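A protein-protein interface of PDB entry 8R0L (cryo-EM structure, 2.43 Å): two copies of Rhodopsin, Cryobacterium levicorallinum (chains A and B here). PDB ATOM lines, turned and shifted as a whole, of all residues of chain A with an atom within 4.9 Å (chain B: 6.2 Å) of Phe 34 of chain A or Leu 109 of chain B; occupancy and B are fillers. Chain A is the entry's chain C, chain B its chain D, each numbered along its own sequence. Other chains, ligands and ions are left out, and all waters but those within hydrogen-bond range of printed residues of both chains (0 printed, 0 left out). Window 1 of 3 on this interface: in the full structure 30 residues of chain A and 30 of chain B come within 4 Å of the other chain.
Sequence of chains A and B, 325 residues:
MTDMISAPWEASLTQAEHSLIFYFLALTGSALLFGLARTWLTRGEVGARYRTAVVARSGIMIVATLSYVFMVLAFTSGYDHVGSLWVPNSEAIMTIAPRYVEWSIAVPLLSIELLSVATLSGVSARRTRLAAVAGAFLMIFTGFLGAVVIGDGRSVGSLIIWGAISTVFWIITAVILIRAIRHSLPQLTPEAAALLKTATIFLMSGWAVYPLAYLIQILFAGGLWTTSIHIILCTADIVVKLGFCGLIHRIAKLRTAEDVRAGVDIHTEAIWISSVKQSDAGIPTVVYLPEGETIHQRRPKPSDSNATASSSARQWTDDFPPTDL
Of chain B, only Val 55 (3.5 Å), Gly 59 (3.5 Å) and Leu 109 (3.7 Å) come within 4 Å of Phe 34 of chain A. Of the printed residues of chain B, Ala 37 of chain A touches Ile 62 (3.5 Å). Of the printed residues of chain B, Arg 38 of chain A touches Val 55 (3.5 Å). Ala 56 of chain B touches none of the printed residues of chain A. Leu 109 of chain B touches just one residue of chain A: Phe 34 (3.7 Å). Leu 110 of chain B touches none of the printed residues of chain A. The nearest printed residue of chain A that does not touch Leu 109 of chain B is Ser 30 of chain A (7.4 Å). The nearest printed residue of chain A that does not touch Val 63 of chain B is Phe 34 of chain A (4.5 Å).
O of Leu 242 of chain A is in hydrogen-bond range of NH1 of Arg 38 of chain A (3.3 Å).
Among the printed residues, merely in contact across the chains: Ser 30 of chain A with Val 63 of chain B (3.7 Å), Ala 31 of chain A with Ile 105 of chain B (3.98 Å), Leu 33 of chain A with Ile 62 of chain B (3.5 Å), Phe 34 of chain A with Val 55 of chain B (3.5 Å), Phe 34 of chain A with Gly 59 of chain B (3.5 Å), Phe 34 of chain A with Leu 109 of chain B (3.7 Å), Ala 37 of chain A with Ile 62 of chain B (3.5 Å) and Arg 38 of chain A with Val 55 of chain B (3.5 Å).
Hydrophobic or aromatic side chains of chain B that line the printed part of chain A: Val 55, Ile 62, Val 63, Ile 105 and Leu 109. Hydrophobic or aromatic side chains of chain A that line the printed part of chain B: Ala 31, Leu 33, Phe 34 and Ala 37. Among the printed residues, 8 pairs touch across the chains. Among the printed residues, no Asp or Glu carboxylate lies within 4 Å of a Lys or Arg side-chain nitrogen of the other chain.
No position is printed for both chains. Of the 8 pairs that touch across the chains among the printed residues, none has its exchanged pair printed and touching as well.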
ATOM      1  N   SER A  30      35.263  -4.796   1.060  1.00  0.00           N
ATOM      2  CA  SER A  30      34.585  -5.251  -0.128  1.00  0.00           C
ATOM      3  C   SER A  30      33.111  -5.506   0.153  1.00  0.00           C
ATOM      4  O   SER A  30      32.265  -5.050  -0.613  1.00  0.00           O
ATOM      5  CB  SER A  30      35.261  -6.499  -0.588  1.00  0.00           C
ATOM      6  OG  SER A  30      36.617  -6.217  -0.876  1.00  0.00           O
ATOM      7  N   ALA A  31      32.839  -6.233   1.241  1.00  0.00           N
ATOM      8  CA  ALA A  31      31.482  -6.568   1.611  1.00  0.00           C
ATOM      9  C   ALA A  31      30.692  -5.296   1.905  1.00  0.00           C
ATOM     10  O   ALA A  31      29.523  -5.219   1.569  1.00  0.00           O
ATOM     11  CB  ALA A  31      31.492  -7.512   2.769  1.00  0.00           C
ATOM     12  N   LEU A  32      31.338  -4.293   2.484  1.00  0.00           N
ATOM     13  CA  LEU A  32      30.636  -3.089   2.861  1.00  0.00           C
ATOM     14  C   LEU A  32      30.431  -2.198   1.649  1.00  0.00           C
ATOM     15  O   LEU A  32      29.550  -1.345   1.682  1.00  0.00           O
ATOM     16  CB  LEU A  32      31.414  -2.358   3.955  1.00  0.00           C
ATOM     17  CG  LEU A  32      31.637  -3.168   5.224  1.00  0.00           C
ATOM     18  CD1 LEU A  32      32.680  -2.498   6.110  1.00  0.00           C
ATOM     19  CD2 LEU A  32      30.347  -3.373   5.976  1.00  0.00           C
ATOM     20  N   LEU A  33      31.266  -2.348   0.624  1.00  0.00           N
ATOM     21  CA  LEU A  33      31.096  -1.583  -0.600  1.00  0.00           C
ATOM     22  C   LEU A  33      29.976  -2.201  -1.446  1.00  0.00           C
ATOM     23  O   LEU A  33      29.204  -1.488  -2.076  1.00  0.00           O
ATOM     24  CB  LEU A  33      32.439  -1.538  -1.325  1.00  0.00           C
ATOM     25  CG  LEU A  33      32.518  -0.562  -2.494  1.00  0.00           C
ATOM     26  CD1 LEU A  33      32.158   0.865  -2.097  1.00  0.00           C
ATOM     27  CD2 LEU A  33      33.913  -0.590  -3.074  1.00  0.00           C
ATOM     28  N   PHE A  34      29.842  -3.523  -1.397  1.00  0.00           N
ATOM     29  CA  PHE A  34      28.669  -4.176  -1.932  1.00  0.00           C
ATOM     30  C   PHE A  34      27.426  -3.715  -1.175  1.00  0.00           C
ATOM     31  O   PHE A  34      26.393  -3.460  -1.783  1.00  0.00           O
ATOM     32  CB  PHE A  34      28.841  -5.690  -1.854  1.00  0.00           C
ATOM     33  CG  PHE A  34      27.546  -6.440  -1.954  1.00  0.00           C
ATOM     34  CD1 PHE A  34      26.750  -6.345  -3.090  1.00  0.00           C
ATOM     35  CD2 PHE A  34      27.106  -7.221  -0.902  1.00  0.00           C
ATOM     36  CE1 PHE A  34      25.550  -7.034  -3.173  1.00  0.00           C
ATOM     37  CE2 PHE A  34      25.899  -7.899  -0.991  1.00  0.00           C
ATOM     38  CZ  PHE A  34      25.123  -7.802  -2.120  1.00  0.00           C
ATOM     39  N   GLY A  35      27.531  -3.619   0.151  1.00  0.00           N
ATOM     40  CA  GLY A  35      26.420  -3.220   0.981  1.00  0.00           C
ATOM     41  C   GLY A  35      25.975  -1.800   0.681  1.00  0.00           C
ATOM     42  O   GLY A  35      24.800  -1.487   0.784  1.00  0.00           O
ATOM     43  N   LEU A  36      26.911  -0.961   0.286  1.00  0.00           N
ATOM     44  CA  LEU A  36      26.590   0.396  -0.091  1.00  0.00           C
ATOM     45  C   LEU A  36      25.858   0.417  -1.421  1.00  0.00           C
ATOM     46  O   LEU A  36      24.902   1.152  -1.591  1.00  0.00           O
ATOM     47  CB  LEU A  36      27.888   1.194  -0.173  1.00  0.00           C
ATOM     48  CG  LEU A  36      27.719   2.662  -0.561  1.00  0.00           C
ATOM     49  CD1 LEU A  36      26.782   3.415   0.393  1.00  0.00           C
ATOM     50  CD2 LEU A  36      29.081   3.316  -0.586  1.00  0.00           C
ATOM     51  N   ALA A  37      26.319  -0.374  -2.369  1.00  0.00           N
ATOM     52  CA  ALA A  37      25.672  -0.442  -3.664  1.00  0.00           C
ATOM     53  C   ALA A  37      24.250  -0.998  -3.538  1.00  0.00           C
ATOM     54  O   ALA A  37      23.343  -0.489  -4.175  1.00  0.00           O
ATOM     55  CB  ALA A  37      26.521  -1.279  -4.575  1.00  0.00           C
ATOM     56  N   ARG A  38      24.058  -2.000  -2.695  1.00  0.00           N
ATOM     57  CA  ARG A  38      22.764  -2.599  -2.452  1.00  0.00           C
ATOM     58  C   ARG A  38      21.796  -1.576  -1.855  1.00  0.00           C
ATOM     59  O   ARG A  38      20.613  -1.545  -2.171  1.00  0.00           O
ATOM     60  CB  ARG A  38      23.001  -3.781  -1.516  1.00  0.00           C
ATOM     61  CG  ARG A  38      21.774  -4.612  -1.214  1.00  0.00           C
ATOM     62  CD  ARG A  38      21.751  -4.948   0.249  1.00  0.00           C
ATOM     63  NE  ARG A  38      21.745  -6.351   0.580  1.00  0.00           N
ATOM     64  CZ  ARG A  38      21.683  -6.784   1.834  1.00  0.00           C
ATOM     65  NH1 ARG A  38      22.452  -6.244   2.769  1.00  0.00           N
ATOM     66  NH2 ARG A  38      20.892  -7.811   2.125  1.00  0.00           N
ATOM     67  N   LEU A 242      25.868  -6.114   7.325  1.00  0.00           N
ATOM     68  CA  LEU A 242      25.203  -6.655   6.144  1.00  0.00           C
ATOM     69  C   LEU A 242      23.954  -7.420   6.560  1.00  0.00           C
ATOM     70  O   LEU A 242      22.930  -7.278   5.905  1.00  0.00           O
ATOM     71  CB  LEU A 242      26.127  -7.568   5.341  1.00  0.00           C
ATOM     72  CG  LEU A 242      27.047  -6.899   4.324  1.00  0.00           C
ATOM     73  CD1 LEU A 242      27.719  -7.967   3.482  1.00  0.00           C
ATOM     74  CD2 LEU A 242      26.308  -5.952   3.393  1.00  0.00           C
ATOM     75  N   VAL B  55      21.460  -6.492  -7.994  1.00  0.00           N
ATOM     76  CA  VAL B  55      22.226  -6.147  -6.816  1.00  0.00           C
ATOM     77  C   VAL B  55      23.455  -7.061  -6.714  1.00  0.00           C
ATOM     78  O   VAL B  55      24.565  -6.589  -6.494  1.00  0.00           O
ATOM     79  CB  VAL B  55      21.314  -6.222  -5.568  1.00  0.00           C
ATOM     80  CG1 VAL B  55      22.105  -6.201  -4.265  1.00  0.00           C
ATOM     81  CG2 VAL B  55      20.284  -5.101  -5.567  1.00  0.00           C
ATOM     82  N   ALA B  56      23.235  -8.364  -6.856  1.00  0.00           N
ATOM     83  CA  ALA B  56      24.309  -9.333  -6.908  1.00  0.00           C
ATOM     84  C   ALA B  56      25.313  -8.955  -7.998  1.00  0.00           C
ATOM     85  O   ALA B  56      26.500  -8.815  -7.728  1.00  0.00           O
ATOM     86  CB  ALA B  56      23.737 -10.706  -7.136  1.00  0.00           C
ATOM     87  N   ARG B  57      24.826  -8.726  -9.208  1.00  0.00           N
ATOM     88  CA  ARG B  57      25.688  -8.384 -10.311  1.00  0.00           C
ATOM     89  C   ARG B  57      26.470  -7.107 -10.028  1.00  0.00           C
ATOM     90  O   ARG B  57      27.667  -7.059 -10.280  1.00  0.00           O
ATOM     91  CB  ARG B  57      24.858  -8.287 -11.582  1.00  0.00           C
ATOM     92  CG  ARG B  57      25.685  -8.107 -12.844  1.00  0.00           C
ATOM     93  CD  ARG B  57      24.764  -8.110 -14.042  1.00  0.00           C
ATOM     94  NE  ARG B  57      23.694  -9.106 -13.921  1.00  0.00           N
ATOM     95  CZ  ARG B  57      22.395  -8.843 -13.757  1.00  0.00           C
ATOM     96  NH1 ARG B  57      21.903  -7.618 -13.907  1.00  0.00           N
ATOM     97  NH2 ARG B  57      21.609  -9.835 -13.389  1.00  0.00           N
ATOM     98  N   SER B  58      25.825  -6.076  -9.507  1.00  0.00           N
ATOM     99  CA  SER B  58      26.534  -4.857  -9.153  1.00  0.00           C
ATOM    100  C   SER B  58      27.655  -5.145  -8.162  1.00  0.00           C
ATOM    101  O   SER B  58      28.738  -4.588  -8.285  1.00  0.00           O
ATOM    102  CB  SER B  58      25.607  -3.826  -8.581  1.00  0.00           C
ATOM    103  OG  SER B  58      24.530  -3.600  -9.469  1.00  0.00           O
ATOM    104  N   GLY B  59      27.382  -6.008  -7.185  1.00  0.00           N
ATOM    105  CA  GLY B  59      28.371  -6.357  -6.181  1.00  0.00           C
ATOM    106  C   GLY B  59      29.532  -7.139  -6.772  1.00  0.00           C
ATOM    107  O   GLY B  59      30.686  -6.838  -6.495  1.00  0.00           O
ATOM    108  N   ILE B  60      29.213  -8.099  -7.640  1.00  0.00           N
ATOM    109  CA  ILE B  60      30.252  -8.822  -8.351  1.00  0.00           C
ATOM    110  C   ILE B  60      31.160  -7.845  -9.096  1.00  0.00           C
ATOM    111  O   ILE B  60      32.363  -7.993  -9.032  1.00  0.00           O
ATOM    112  CB  ILE B  60      29.675  -9.909  -9.256  1.00  0.00           C
ATOM    113  CG1 ILE B  60      28.915 -10.958  -8.459  1.00  0.00           C
ATOM    114  CG2 ILE B  60      30.787 -10.566 -10.054  1.00  0.00           C
ATOM    115  CD1 ILE B  60      27.875 -11.715  -9.277  1.00  0.00           C
ATOM    116  N   ILE B  62      31.718  -4.495  -8.647  1.00  0.00           N
ATOM    117  CA  ILE B  62      32.433  -3.529  -7.823  1.00  0.00           C
ATOM    118  C   ILE B  62      33.574  -4.228  -7.078  1.00  0.00           C
ATOM    119  O   ILE B  62      34.697  -3.741  -7.062  1.00  0.00           O
ATOM    120  CB  ILE B  62      31.492  -2.805  -6.844  1.00  0.00           C
ATOM    121  CG1 ILE B  62      30.401  -2.028  -7.568  1.00  0.00           C
ATOM    122  CG2 ILE B  62      32.261  -1.869  -5.932  1.00  0.00           C
ATOM    123  CD1 ILE B  62      29.369  -1.429  -6.624  1.00  0.00           C
ATOM    124  N   VAL B  63      33.311  -5.382  -6.477  1.00  0.00           N
ATOM    125  CA  VAL B  63      34.368  -6.008  -5.703  1.00  0.00           C
ATOM    126  C   VAL B  63      35.480  -6.424  -6.656  1.00  0.00           C
ATOM    127  O   VAL B  63      36.649  -6.259  -6.336  1.00  0.00           O
ATOM    128  CB  VAL B  63      33.898  -7.173  -4.811  1.00  0.00           C
ATOM    129  CG1 VAL B  63      32.774  -6.729  -3.875  1.00  0.00           C
ATOM    130  CG2 VAL B  63      33.480  -8.397  -5.614  1.00  0.00           C
ATOM    131  N   SER B 104      35.725 -14.396  -2.756  1.00  0.00           N
ATOM    132  CA  SER B 104      35.075 -14.723  -1.506  1.00  0.00           C
ATOM    133  C   SER B 104      33.727 -14.030  -1.447  1.00  0.00           C
ATOM    134  O   SER B 104      32.790 -14.591  -0.896  1.00  0.00           O
ATOM    135  CB  SER B 104      35.972 -14.394  -0.384  1.00  0.00           C
ATOM    136  OG  SER B 104      36.852 -15.481  -0.204  1.00  0.00           O
ATOM    137  N   ILE B 105      33.635 -12.860  -2.076  1.00  0.00           N
ATOM    138  CA  ILE B 105      32.375 -12.160  -2.178  1.00  0.00           C
ATOM    139  C   ILE B 105      31.629 -12.642  -3.416  1.00  0.00           C
ATOM    140  O   ILE B 105      30.452 -12.977  -3.327  1.00  0.00           O
ATOM    141  CB  ILE B 105      32.578 -10.639  -2.190  1.00  0.00           C
ATOM    142  CG1 ILE B 105      33.467 -10.159  -1.040  1.00  0.00           C
ATOM    143  CG2 ILE B 105      31.235  -9.940  -2.157  1.00  0.00           C
ATOM    144  CD1 ILE B 105      32.833 -10.327   0.292  1.00  0.00           C
ATOM    145  N   ALA B 106      32.334 -12.724  -4.546  1.00  0.00           N
ATOM    146  CA  ALA B 106      31.738 -12.879  -5.866  1.00  0.00           C
ATOM    147  C   ALA B 106      31.192 -14.275  -6.126  1.00  0.00           C
ATOM    148  O   ALA B 106      30.196 -14.396  -6.820  1.00  0.00           O
ATOM    149  CB  ALA B 106      32.735 -12.513  -6.921  1.00  0.00           C
ATOM    150  N   VAL B 107      31.804 -15.328  -5.618  1.00  0.00           N
ATOM    151  CA  VAL B 107      31.263 -16.646  -5.921  1.00  0.00           C
ATOM    152  C   VAL B 107      29.950 -16.848  -5.166  1.00  0.00           C
ATOM    153  O   VAL B 107      29.003 -17.406  -5.707  1.00  0.00           O
ATOM    154  CB  VAL B 107      32.305 -17.752  -5.673  1.00  0.00           C
ATOM    155  CG1 VAL B 107      31.751 -19.138  -5.913  1.00  0.00           C
ATOM    156  CG2 VAL B 107      33.529 -17.492  -6.540  1.00  0.00           C
ATOM    157  N   PRO B 108      29.861 -16.434  -3.884  1.00  0.00           N
ATOM    158  CA  PRO B 108      28.585 -16.324  -3.162  1.00  0.00           C
ATOM    159  C   PRO B 108      27.509 -15.496  -3.864  1.00  0.00           C
ATOM    160  O   PRO B 108      26.371 -15.946  -3.942  1.00  0.00           O
ATOM    161  CB  PRO B 108      29.047 -15.650  -1.867  1.00  0.00           C
ATOM    162  CG  PRO B 108      30.357 -16.304  -1.642  1.00  0.00           C
ATOM    163  CD  PRO B 108      30.996 -16.140  -3.000  1.00  0.00           C
ATOM    164  N   LEU B 109      27.921 -14.367  -4.460  1.00  0.00           N
ATOM    165  CA  LEU B 109      27.019 -13.457  -5.145  1.00  0.00           C
ATOM    166  C   LEU B 109      26.531 -14.032  -6.460  1.00  0.00           C
ATOM    167  O   LEU B 109      25.399 -13.775  -6.842  1.00  0.00           O
ATOM    168  CB  LEU B 109      27.678 -12.093  -5.361  1.00  0.00           C
ATOM    169  CG  LEU B 109      27.665 -11.164  -4.139  1.00  0.00           C
ATOM    170  CD1 LEU B 109      28.185  -9.800  -4.512  1.00  0.00           C
ATOM    171  CD2 LEU B 109      26.271 -11.003  -3.527  1.00  0.00           C
ATOM    172  N   LEU B 110      27.340 -14.859  -7.114  1.00  0.00           N
ATOM    173  CA  LEU B 110      26.931 -15.519  -8.337  1.00  0.00           C
ATOM    174  C   LEU B 110      25.889 -16.573  -8.032  1.00  0.00           C
ATOM    175  O   LEU B 110      25.009 -16.805  -8.836  1.00  0.00           O
ATOM    176  CB  LEU B 110      28.153 -16.128  -9.011  1.00  0.00           C
ATOM    177  CG  LEU B 110      29.092 -15.093  -9.630  1.00  0.00           C
ATOM    178  CD1 LEU B 110      30.511 -15.650  -9.829  1.00  0.00           C
ATOM    179  CD2 LEU B 110      28.547 -14.599 -10.964  1.00  0.00           C
ATOM    180  N   SER B 111      26.001 -17.221  -6.887  1.00  0.00           N
ATOM    181  CA  SER B 111      25.029 -18.218  -6.486  1.00  0.00           C
ATOM    182  C   SER B 111      23.681 -17.525  -6.291  1.00  0.00           C
ATOM    183  O   SER B 111      22.640 -18.032  -6.726  1.00  0.00           O
ATOM    184  CB  SER B 111      25.489 -18.913  -5.221  1.00  0.00           C
ATOM    185  OG  SER B 111      26.840 -19.304  -5.331  1.00  0.00           O
ATOM    186  N   ILE B 112      23.742 -16.354  -5.645  1.00  0.00           N
ATOM    187  CA  ILE B 112      22.565 -15.570  -5.340  1.00  0.00           C
ATOM    188  C   ILE B 112      21.902 -15.080  -6.615  1.00  0.00           C
ATOM    189  O   ILE B 112      20.687 -15.168  -6.703  1.00  0.00           O
ATOM    190  CB  ILE B 112      22.921 -14.427  -4.378  1.00  0.00           C
ATOM    191  CG1 ILE B 112      23.026 -14.947  -2.950  1.00  0.00           C
ATOM    192  CG2 ILE B 112      21.939 -13.264  -4.431  1.00  0.00           C
ATOM    193  CD1 ILE B 112      23.900 -14.034  -2.137  1.00  0.00           C
ATOM    194  N   GLU B 113      22.698 -14.604  -7.569  1.00  0.00           N
ATOM    195  CA  GLU B 113      22.225 -14.151  -8.863  1.00  0.00           C
ATOM    196  C   GLU B 113      21.518 -15.265  -9.642  1.00  0.00           C
ATOM    197  O   GLU B 113      20.428 -15.035 -10.168  1.00  0.00           O
ATOM    198  CB  GLU B 113      23.401 -13.582  -9.645  1.00  0.00           C
ATOM    199  CG  GLU B 113      22.983 -12.604 -10.716  1.00  0.00           C
ATOM    200  CD  GLU B 113      24.143 -12.163 -11.596  1.00  0.00           C
ATOM    201  OE1 GLU B 113      23.897 -11.507 -12.644  1.00  0.00           O
ATOM    202  OE2 GLU B 113      25.308 -12.469 -11.220  1.00  0.00           O
ATOM    203  N   LEU B 114      22.093 -16.466  -9.694  1.00  0.00           N
ATOM    204  CA  LEU B 114      21.448 -17.574 -10.374  1.00  0.00           C
ATOM    205  C   LEU B 114      20.102 -17.917  -9.735  1.00  0.00           C
ATOM    206  O   LEU B 114      19.176 -18.296 -10.438  1.00  0.00           O
ATOM    207  CB  LEU B 114      22.408 -18.761 -10.353  1.00  0.00           C
ATOM    208  CG  LEU B 114      21.986 -19.992 -11.136  1.00  0.00           C
ATOM    209  CD1 LEU B 114      22.066 -19.750 -12.631  1.00  0.00           C
ATOM    210  CD2 LEU B 114      22.873 -21.153 -10.751  1.00  0.00           C
ATOM    211  N   VAL B 133      25.660 -19.629  -0.208  1.00  0.00           N
ATOM    212  CA  VAL B 133      26.604 -18.598   0.192  1.00  0.00           C
ATOM    213  C   VAL B 133      27.641 -19.149   1.162  1.00  0.00           C
ATOM    214  O   VAL B 133      28.776 -18.690   1.176  1.00  0.00           O
ATOM    215  CB  VAL B 133      25.857 -17.393   0.787  1.00  0.00           C
ATOM    216  CG1 VAL B 133      26.784 -16.451   1.544  1.00  0.00           C
ATOM    217  CG2 VAL B 133      25.114 -16.645  -0.316  1.00  0.00           C
